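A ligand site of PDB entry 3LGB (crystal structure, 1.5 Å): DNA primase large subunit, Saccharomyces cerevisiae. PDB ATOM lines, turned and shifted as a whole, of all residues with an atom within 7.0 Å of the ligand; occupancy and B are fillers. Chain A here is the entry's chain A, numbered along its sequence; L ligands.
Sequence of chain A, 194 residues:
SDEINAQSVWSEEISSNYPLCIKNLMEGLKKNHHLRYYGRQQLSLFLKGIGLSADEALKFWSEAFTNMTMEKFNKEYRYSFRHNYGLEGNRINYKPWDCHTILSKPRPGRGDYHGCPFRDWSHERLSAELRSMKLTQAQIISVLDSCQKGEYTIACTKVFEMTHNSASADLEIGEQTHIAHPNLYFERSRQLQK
An iron atom (FE1) of the ligand is bound by the side-chain sulfur (SG) of Cys 99 (2.3 Å).
The side-chain sulfur (SG) of Cys 156 is bound to an iron atom (FE3) of the ligand (2.3 Å).
N of Cys 21 sits close to S1 of the ligand, 3.4 Å away.
The side-chain sulfur (SG) of Cys 21 is bound to an iron atom (FE4) of the ligand (2.3 Å).
An iron atom (FE2) of the ligand is bound by the side-chain sulfur (SG) of Cys 116 (2.3 Å).
SG of Cys 99 lies close to N of His 181.
N of Cys 99 sits at hydrogen-bond distance from O of Ala 180 (3.1 Å).
SG of Cys 116 lies close to N of Phe 118 (3.5 Å).
O of Thr 153 lies within hydrogen-bond range of OG1 of Thr 157, 2.8 Å away.
N of Pro 182 sits close to S2 of the ligand (3.8 Å).
Merely in contact with the ligand: Phe 118 (3.7 Å), Pro 19 (3.8 Å), Ile 102 (3.8 Å), Tyr 152 (3.9 Å), Thr 153 (3.9 Å) and Pro 117 (3.9 Å).
Hydrophobic or aromatic side chains that line the ligand: Pro 19, Ile 102, Pro 117, Phe 118 and Pro 182.
The nearest printed residue that does not touch the ligand is Leu 20 (4.02 Å).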
ATOM      1  N   PRO A  19       3.874  37.208  -5.278  1.00  0.00           N
ATOM      2  CA  PRO A  19       3.185  36.617  -4.132  1.00  0.00           C
ATOM      3  C   PRO A  19       4.168  36.481  -2.962  1.00  0.00           C
ATOM      4  O   PRO A  19       5.380  36.687  -3.131  1.00  0.00           O
ATOM      5  CB  PRO A  19       2.714  35.263  -4.639  1.00  0.00           C
ATOM      6  CG  PRO A  19       3.786  34.885  -5.669  1.00  0.00           C
ATOM      7  CD  PRO A  19       4.219  36.199  -6.311  1.00  0.00           C
ATOM      8  N   LEU A  20       3.649  36.125  -1.782  1.00  0.00           N
ATOM      9  CA  LEU A  20       4.455  36.074  -0.561  1.00  0.00           C
ATOM     10  C   LEU A  20       5.676  35.170  -0.667  1.00  0.00           C
ATOM     11  O   LEU A  20       6.741  35.534  -0.166  1.00  0.00           O
ATOM     12  CB  LEU A  20       3.631  35.694   0.677  1.00  0.00           C
ATOM     13  CG  LEU A  20       2.614  36.701   1.215  1.00  0.00           C
ATOM     14  CD1 LEU A  20       2.160  36.316   2.632  1.00  0.00           C
ATOM     15  CD2 LEU A  20       3.183  38.100   1.268  1.00  0.00           C
ATOM     16  N   CYS A  21       5.547  33.996  -1.297  1.00  0.00           N
ATOM     17  CA  CYS A  21       6.708  33.087  -1.382  1.00  0.00           C
ATOM     18  C   CYS A  21       7.854  33.747  -2.115  1.00  0.00           C
ATOM     19  O   CYS A  21       9.010  33.648  -1.678  1.00  0.00           O
ATOM     20  CB  CYS A  21       6.317  31.753  -2.039  1.00  0.00           C
ATOM     21  SG  CYS A  21       5.536  31.928  -3.659  1.00  0.00           S
ATOM     22  N   ILE A  22       7.546  34.387  -3.267  1.00  0.00           N
ATOM     23  CA  ILE A  22       8.611  35.020  -4.044  1.00  0.00           C
ATOM     24  C   ILE A  22       9.169  36.212  -3.290  1.00  0.00           C
ATOM     25  O   ILE A  22      10.384  36.418  -3.289  1.00  0.00           O
ATOM     26  CB  ILE A  22       8.071  35.399  -5.439  1.00  0.00           C
ATOM     27  CG1 ILE A  22       7.590  34.137  -6.232  1.00  0.00           C
ATOM     28  CG2 ILE A  22       9.128  36.186  -6.225  1.00  0.00           C
ATOM     29  CD1 ILE A  22       8.672  32.978  -6.368  1.00  0.00           C
ATOM     30  N   GLN A  42      13.092  27.242  -6.750  1.00  0.00           N
ATOM     31  CA  GLN A  42      11.785  27.898  -6.760  1.00  0.00           C
ATOM     32  C   GLN A  42      11.851  29.285  -7.386  1.00  0.00           C
ATOM     33  O   GLN A  42      11.033  29.626  -8.245  1.00  0.00           O
ATOM     34  CB  GLN A  42      11.267  27.994  -5.319  1.00  0.00           C
ATOM     35  CG  GLN A  42       9.810  28.510  -5.211  1.00  0.00           C
ATOM     36  CD  GLN A  42       9.254  28.337  -3.814  1.00  0.00           C
ATOM     37  OE1 GLN A  42       9.734  27.495  -3.027  1.00  0.00           O
ATOM     38  NE2 GLN A  42       8.195  29.076  -3.488  1.00  0.00           N
ATOM     39  N   ASP A  98       4.135  25.131  -9.657  1.00  0.00           N
ATOM     40  CA  ASP A  98       2.866  25.637  -9.162  1.00  0.00           C
ATOM     41  C   ASP A  98       2.863  25.462  -7.617  1.00  0.00           C
ATOM     42  O   ASP A  98       3.846  24.946  -7.050  1.00  0.00           O
ATOM     43  CB  ASP A  98       1.680  24.918  -9.810  1.00  0.00           C
ATOM     44  CG  ASP A  98       1.627  23.418  -9.628  1.00  0.00           C
ATOM     45  OD1 ASP A  98       2.551  22.866  -8.986  1.00  0.00           O
ATOM     46  OD2 ASP A  98       0.710  22.787 -10.189  1.00  0.00           O
ATOM     47  N   CYS A  99       1.788  25.924  -6.942  1.00  0.00           N
ATOM     48  CA  CYS A  99       1.745  25.812  -5.479  1.00  0.00           C
ATOM     49  C   CYS A  99       1.811  24.371  -5.021  1.00  0.00           C
ATOM     50  O   CYS A  99       2.507  24.065  -4.051  1.00  0.00           O
ATOM     51  CB  CYS A  99       0.509  26.519  -4.959  1.00  0.00           C
ATOM     52  SG  CYS A  99       0.437  28.252  -5.514  1.00  0.00           S
ATOM     53  N   HIS A 100       1.088  23.477  -5.720  1.00  0.00           N
ATOM     54  CA  HIS A 100       1.129  22.038  -5.396  1.00  0.00           C
ATOM     55  C   HIS A 100       2.579  21.539  -5.373  1.00  0.00           C
ATOM     56  O   HIS A 100       2.987  20.859  -4.430  1.00  0.00           O
ATOM     57  CB  HIS A 100       0.302  21.309  -6.469  1.00  0.00           C
ATOM     58  CG  HIS A 100       0.429  19.826  -6.447  1.00  0.00           C
ATOM     59  ND1 HIS A 100      -0.338  19.061  -5.598  1.00  0.00           N
ATOM     60  CD2 HIS A 100       1.153  19.016  -7.254  1.00  0.00           C
ATOM     61  CE1 HIS A 100      -0.030  17.805  -5.895  1.00  0.00           C
ATOM     62  NE2 HIS A 100       0.855  17.738  -6.891  1.00  0.00           N
ATOM     63  N   ILE A 102       5.423  23.390  -5.131  1.00  0.00           N
ATOM     64  CA  ILE A 102       6.143  24.094  -4.057  1.00  0.00           C
ATOM     65  C   ILE A 102       5.871  23.435  -2.717  1.00  0.00           C
ATOM     66  O   ILE A 102       6.825  23.169  -1.961  1.00  0.00           O
ATOM     67  CB  ILE A 102       5.692  25.570  -4.065  1.00  0.00           C
ATOM     68  CG1 ILE A 102       6.342  26.293  -5.268  1.00  0.00           C
ATOM     69  CG2 ILE A 102       6.068  26.243  -2.732  1.00  0.00           C
ATOM     70  CD1 ILE A 102       5.650  27.628  -5.571  1.00  0.00           C
ATOM     71  N   LEU A 103       4.598  23.146  -2.437  1.00  0.00           N
ATOM     72  CA  LEU A 103       4.212  22.543  -1.154  1.00  0.00           C
ATOM     73  C   LEU A 103       4.769  21.124  -0.987  1.00  0.00           C
ATOM     74  O   LEU A 103       4.969  20.695   0.154  1.00  0.00           O
ATOM     75  CB  LEU A 103       2.675  22.543  -1.024  1.00  0.00           C
ATOM     76  CG  LEU A 103       2.080  23.948  -0.837  1.00  0.00           C
ATOM     77  CD1 LEU A 103       0.583  24.001  -1.218  1.00  0.00           C
ATOM     78  CD2 LEU A 103       2.306  24.481   0.614  1.00  0.00           C
ATOM     79  N   GLY A 115       9.268  27.281  -0.130  1.00  0.00           N
ATOM     80  CA  GLY A 115       8.007  26.847   0.449  1.00  0.00           C
ATOM     81  C   GLY A 115       6.940  27.909   0.276  1.00  0.00           C
ATOM     82  O   GLY A 115       6.984  28.727  -0.647  1.00  0.00           O
ATOM     83  N   CYS A 116       5.922  27.829   1.149  1.00  0.00           N
ATOM     84  CA  CYS A 116       4.782  28.723   1.100  1.00  0.00           C
ATOM     85  C   CYS A 116       4.631  29.389   2.454  1.00  0.00           C
ATOM     86  O   CYS A 116       4.306  28.695   3.410  1.00  0.00           O
ATOM     87  CB  CYS A 116       3.509  27.958   0.746  1.00  0.00           C
ATOM     88  SG  CYS A 116       2.020  28.969   0.864  1.00  0.00           S
ATOM     89  N   PRO A 117       4.782  30.733   2.538  1.00  0.00           N
ATOM     90  CA  PRO A 117       4.649  31.408   3.845  1.00  0.00           C
ATOM     91  C   PRO A 117       3.309  31.184   4.539  1.00  0.00           C
ATOM     92  O   PRO A 117       3.263  31.183   5.784  1.00  0.00           O
ATOM     93  CB  PRO A 117       4.869  32.864   3.495  1.00  0.00           C
ATOM     94  CG  PRO A 117       5.857  32.812   2.327  1.00  0.00           C
ATOM     95  CD  PRO A 117       5.286  31.663   1.503  1.00  0.00           C
ATOM     96  N   PHE A 118       2.221  30.957   3.778  1.00  0.00           N
ATOM     97  CA  PHE A 118       0.924  30.741   4.439  1.00  0.00           C
ATOM     98  C   PHE A 118       0.922  29.461   5.282  1.00  0.00           C
ATOM     99  O   PHE A 118       0.192  29.376   6.258  1.00  0.00           O
ATOM    100  CB  PHE A 118      -0.212  30.753   3.413  1.00  0.00           C
ATOM    101  CG  PHE A 118      -0.343  32.121   2.782  1.00  0.00           C
ATOM    102  CD1 PHE A 118      -0.917  33.180   3.482  1.00  0.00           C
ATOM    103  CD2 PHE A 118       0.134  32.371   1.506  1.00  0.00           C
ATOM    104  CE1 PHE A 118      -1.002  34.467   2.921  1.00  0.00           C
ATOM    105  CE2 PHE A 118       0.038  33.640   0.923  1.00  0.00           C
ATOM    106  CZ  PHE A 118      -0.546  34.686   1.639  1.00  0.00           C
ATOM    107  N   ARG A 119       1.777  28.479   4.900  1.00  0.00           N
ATOM    108  CA  ARG A 119       1.946  27.239   5.676  1.00  0.00           C
ATOM    109  C   ARG A 119       3.135  27.382   6.648  1.00  0.00           C
ATOM    110  O   ARG A 119       3.070  26.919   7.799  1.00  0.00           O
ATOM    111  CB  ARG A 119       2.248  26.092   4.720  1.00  0.00           C
ATOM    112  CG  ARG A 119       2.435  24.745   5.415  1.00  0.00           C
ATOM    113  CD  ARG A 119       3.027  23.683   4.510  1.00  0.00           C
ATOM    114  NE  ARG A 119       4.349  24.093   4.023  1.00  0.00           N
ATOM    115  CZ  ARG A 119       5.031  23.493   3.055  1.00  0.00           C
ATOM    116  NH1 ARG A 119       4.551  22.386   2.473  1.00  0.00           N
ATOM    117  NH2 ARG A 119       6.229  23.935   2.700  1.00  0.00           N
ATOM    118  N   TYR A 152      -3.973  26.925   1.941  1.00  0.00           N
ATOM    119  CA  TYR A 152      -2.947  27.946   1.660  1.00  0.00           C
ATOM    120  C   TYR A 152      -3.211  28.748   0.414  1.00  0.00           C
ATOM    121  O   TYR A 152      -3.075  29.967   0.451  1.00  0.00           O
ATOM    122  CB  TYR A 152      -1.548  27.311   1.636  1.00  0.00           C
ATOM    123  CG  TYR A 152      -1.334  26.449   2.863  1.00  0.00           C
ATOM    124  CD1 TYR A 152      -1.483  26.986   4.144  1.00  0.00           C
ATOM    125  CD2 TYR A 152      -1.033  25.101   2.745  1.00  0.00           C
ATOM    126  CE1 TYR A 152      -1.375  26.177   5.282  1.00  0.00           C
ATOM    127  CE2 TYR A 152      -0.879  24.297   3.865  1.00  0.00           C
ATOM    128  CZ  TYR A 152      -1.068  24.834   5.133  1.00  0.00           C
ATOM    129  OH  TYR A 152      -0.939  24.022   6.235  1.00  0.00           O
ATOM    130  N   THR A 153      -3.653  28.079  -0.673  1.00  0.00           N
ATOM    131  CA  THR A 153      -3.906  28.811  -1.927  1.00  0.00           C
ATOM    132  C   THR A 153      -5.147  29.698  -1.790  1.00  0.00           C
ATOM    133  O   THR A 153      -5.220  30.729  -2.455  1.00  0.00           O
ATOM    134  CB  THR A 153      -3.971  27.897  -3.143  1.00  0.00           C
ATOM    135  OG1 THR A 153      -5.059  26.963  -2.966  1.00  0.00           O
ATOM    136  CG2 THR A 153      -2.636  27.155  -3.384  1.00  0.00           C
ATOM    137  N   ILE A 154      -6.091  29.323  -0.897  1.00  0.00           N
ATOM    138  CA  ILE A 154      -7.242  30.192  -0.637  1.00  0.00           C
ATOM    139  C   ILE A 154      -6.759  31.438   0.130  1.00  0.00           C
ATOM    140  O   ILE A 154      -7.163  32.549  -0.210  1.00  0.00           O
ATOM    141  CB  ILE A 154      -8.374  29.460   0.103  1.00  0.00           C
ATOM    142  CG1 ILE A 154      -8.939  28.347  -0.806  1.00  0.00           C
ATOM    143  CG2 ILE A 154      -9.478  30.460   0.550  1.00  0.00           C
ATOM    144  CD1 ILE A 154     -10.159  27.571  -0.177  1.00  0.00           C
ATOM    145  N   ALA A 155      -5.863  31.248   1.128  1.00  0.00           N
ATOM    146  CA  ALA A 155      -5.313  32.377   1.887  1.00  0.00           C
ATOM    147  C   ALA A 155      -4.599  33.325   0.913  1.00  0.00           C
ATOM    148  O   ALA A 155      -4.762  34.547   0.982  1.00  0.00           O
ATOM    149  CB  ALA A 155      -4.345  31.874   2.947  1.00  0.00           C
ATOM    150  N   CYS A 156      -3.814  32.753  -0.010  1.00  0.00           N
ATOM    151  CA  CYS A 156      -3.049  33.521  -0.991  1.00  0.00           C
ATOM    152  C   CYS A 156      -3.997  34.270  -1.941  1.00  0.00           C
ATOM    153  O   CYS A 156      -3.783  35.450  -2.233  1.00  0.00           O
ATOM    154  CB  CYS A 156      -2.114  32.581  -1.755  1.00  0.00           C
ATOM    155  SG  CYS A 156      -0.940  33.435  -2.825  1.00  0.00           S
ATOM    156  N   THR A 157      -5.077  33.598  -2.371  1.00  0.00           N
ATOM    157  CA  THR A 157      -6.073  34.241  -3.253  1.00  0.00           C
ATOM    158  C   THR A 157      -6.743  35.411  -2.517  1.00  0.00           C
ATOM    159  O   THR A 157      -6.966  36.476  -3.125  1.00  0.00           O
ATOM    160  CB  THR A 157      -7.072  33.202  -3.722  1.00  0.00           C
ATOM    161  OG1 THR A 157      -6.399  32.213  -4.502  1.00  0.00           O
ATOM    162  CG2 THR A 157      -8.173  33.814  -4.567  1.00  0.00           C
ATOM    163  N   ILE A 179      -6.244  31.279  -7.314  1.00  0.00           N
ATOM    164  CA  ILE A 179      -4.853  31.273  -7.785  1.00  0.00           C
ATOM    165  C   ILE A 179      -4.090  30.138  -7.112  1.00  0.00           C
ATOM    166  O   ILE A 179      -4.190  29.950  -5.914  1.00  0.00           O
ATOM    167  CB  ILE A 179      -4.172  32.664  -7.664  1.00  0.00           C
ATOM    168  CG1 ILE A 179      -5.002  33.759  -8.364  1.00  0.00           C
ATOM    169  CG2 ILE A 179      -2.720  32.621  -8.201  1.00  0.00           C
ATOM    170  CD1 ILE A 179      -4.607  35.242  -7.971  1.00  0.00           C
ATOM    171  N   ALA A 180      -3.407  29.325  -7.909  1.00  0.00           N
ATOM    172  CA  ALA A 180      -2.672  28.209  -7.344  1.00  0.00           C
ATOM    173  C   ALA A 180      -1.365  28.013  -8.143  1.00  0.00           C
ATOM    174  O   ALA A 180      -0.842  26.898  -8.315  1.00  0.00           O
ATOM    175  CB  ALA A 180      -3.530  26.958  -7.329  1.00  0.00           C
ATOM    176  N   HIS A 181      -0.771  29.162  -8.507  1.00  0.00           N
ATOM    177  CA  HIS A 181       0.521  29.147  -9.184  1.00  0.00           C
ATOM    178  C   HIS A 181       1.119  30.541  -8.983  1.00  0.00           C
ATOM    179  O   HIS A 181       0.479  31.524  -9.350  1.00  0.00           O
ATOM    180  CB  HIS A 181       0.336  28.891 -10.695  1.00  0.00           C
ATOM    181  CG  HIS A 181       1.601  28.495 -11.407  1.00  0.00           C
ATOM    182  ND1 HIS A 181       2.776  29.286 -11.334  1.00  0.00           N
ATOM    183  CD2 HIS A 181       1.852  27.439 -12.209  1.00  0.00           C
ATOM    184  CE1 HIS A 181       3.674  28.646 -12.083  1.00  0.00           C
ATOM    185  NE2 HIS A 181       3.159  27.532 -12.628  1.00  0.00           N
ATOM    186  N   PRO A 182       2.354  30.651  -8.442  1.00  0.00           N
ATOM    187  CA  PRO A 182       2.935  32.002  -8.236  1.00  0.00           C
ATOM    188  C   PRO A 182       3.021  32.809  -9.541  1.00  0.00           C
ATOM    189  O   PRO A 182       2.905  34.036  -9.490  1.00  0.00           O
ATOM    190  CB  PRO A 182       4.359  31.728  -7.718  1.00  0.00           C
ATOM    191  CG  PRO A 182       4.356  30.287  -7.280  1.00  0.00           C
ATOM    192  CD  PRO A 182       3.235  29.566  -7.960  1.00  0.00           C
ATOM    193  N   ASN A 183       3.266  32.160 -10.680  1.00  0.00           N
ATOM    194  CA  ASN A 183       3.359  32.899 -11.946  1.00  0.00           C
ATOM    195  C   ASN A 183       2.001  33.434 -12.370  1.00  0.00           C
ATOM    196  O   ASN A 183       1.943  34.503 -13.018  1.00  0.00           O
ATOM    197  CB  ASN A 183       3.996  32.056 -13.040  1.00  0.00           C
ATOM    198  CG  ASN A 183       5.475  31.914 -12.795  1.00  0.00           C
ATOM    199  OD1 ASN A 183       5.953  31.026 -12.090  1.00  0.00           O
ATOM    200  ND2 ASN A 183       6.235  32.886 -13.319  1.00  0.00           N
ATOM    201  N   TYR A 185      -0.283  34.433 -10.169  1.00  0.00           N
ATOM    202  CA  TYR A 185      -0.490  35.542  -9.258  1.00  0.00           C
ATOM    203  C   TYR A 185       0.234  36.758  -9.850  1.00  0.00           C
ATOM    204  O   TYR A 185      -0.342  37.838  -9.944  1.00  0.00           O
ATOM    205  CB  TYR A 185       0.154  35.168  -7.917  1.00  0.00           C
ATOM    206  CG  TYR A 185      -0.137  36.095  -6.749  1.00  0.00           C
ATOM    207  CD1 TYR A 185      -0.892  35.655  -5.671  1.00  0.00           C
ATOM    208  CD2 TYR A 185       0.449  37.359  -6.678  1.00  0.00           C
ATOM    209  CE1 TYR A 185      -1.159  36.487  -4.592  1.00  0.00           C
ATOM    210  CE2 TYR A 185       0.216  38.189  -5.578  1.00  0.00           C
ATOM    211  CZ  TYR A 185      -0.568  37.733  -4.532  1.00  0.00           C
ATOM    212  OH  TYR A 185      -0.776  38.514  -3.439  1.00  0.00           O
HETATM  213 FE1  LIG L   1       1.321  29.486  -3.838  1.00  0.00          FE
HETATM  214 FE2  LIG L   1       1.954  29.980  -1.218  1.00  0.00          FE
HETATM  215 FE3  LIG L   1       0.774  31.914  -2.768  1.00  0.00          FE
HETATM  216 FE4  LIG L   1       3.398  31.177  -3.230  1.00  0.00          FE
HETATM  217  S1  LIG L   1       2.594  32.271  -1.306  1.00  0.00           S
HETATM  218  S2  LIG L   1       1.783  31.577  -4.838  1.00  0.00           S
HETATM  219  S3  LIG L   1       3.288  28.851  -2.765  1.00  0.00           S
HETATM  220  S4  LIG L   1      -0.170  29.869  -2.089  1.00  0.00           S
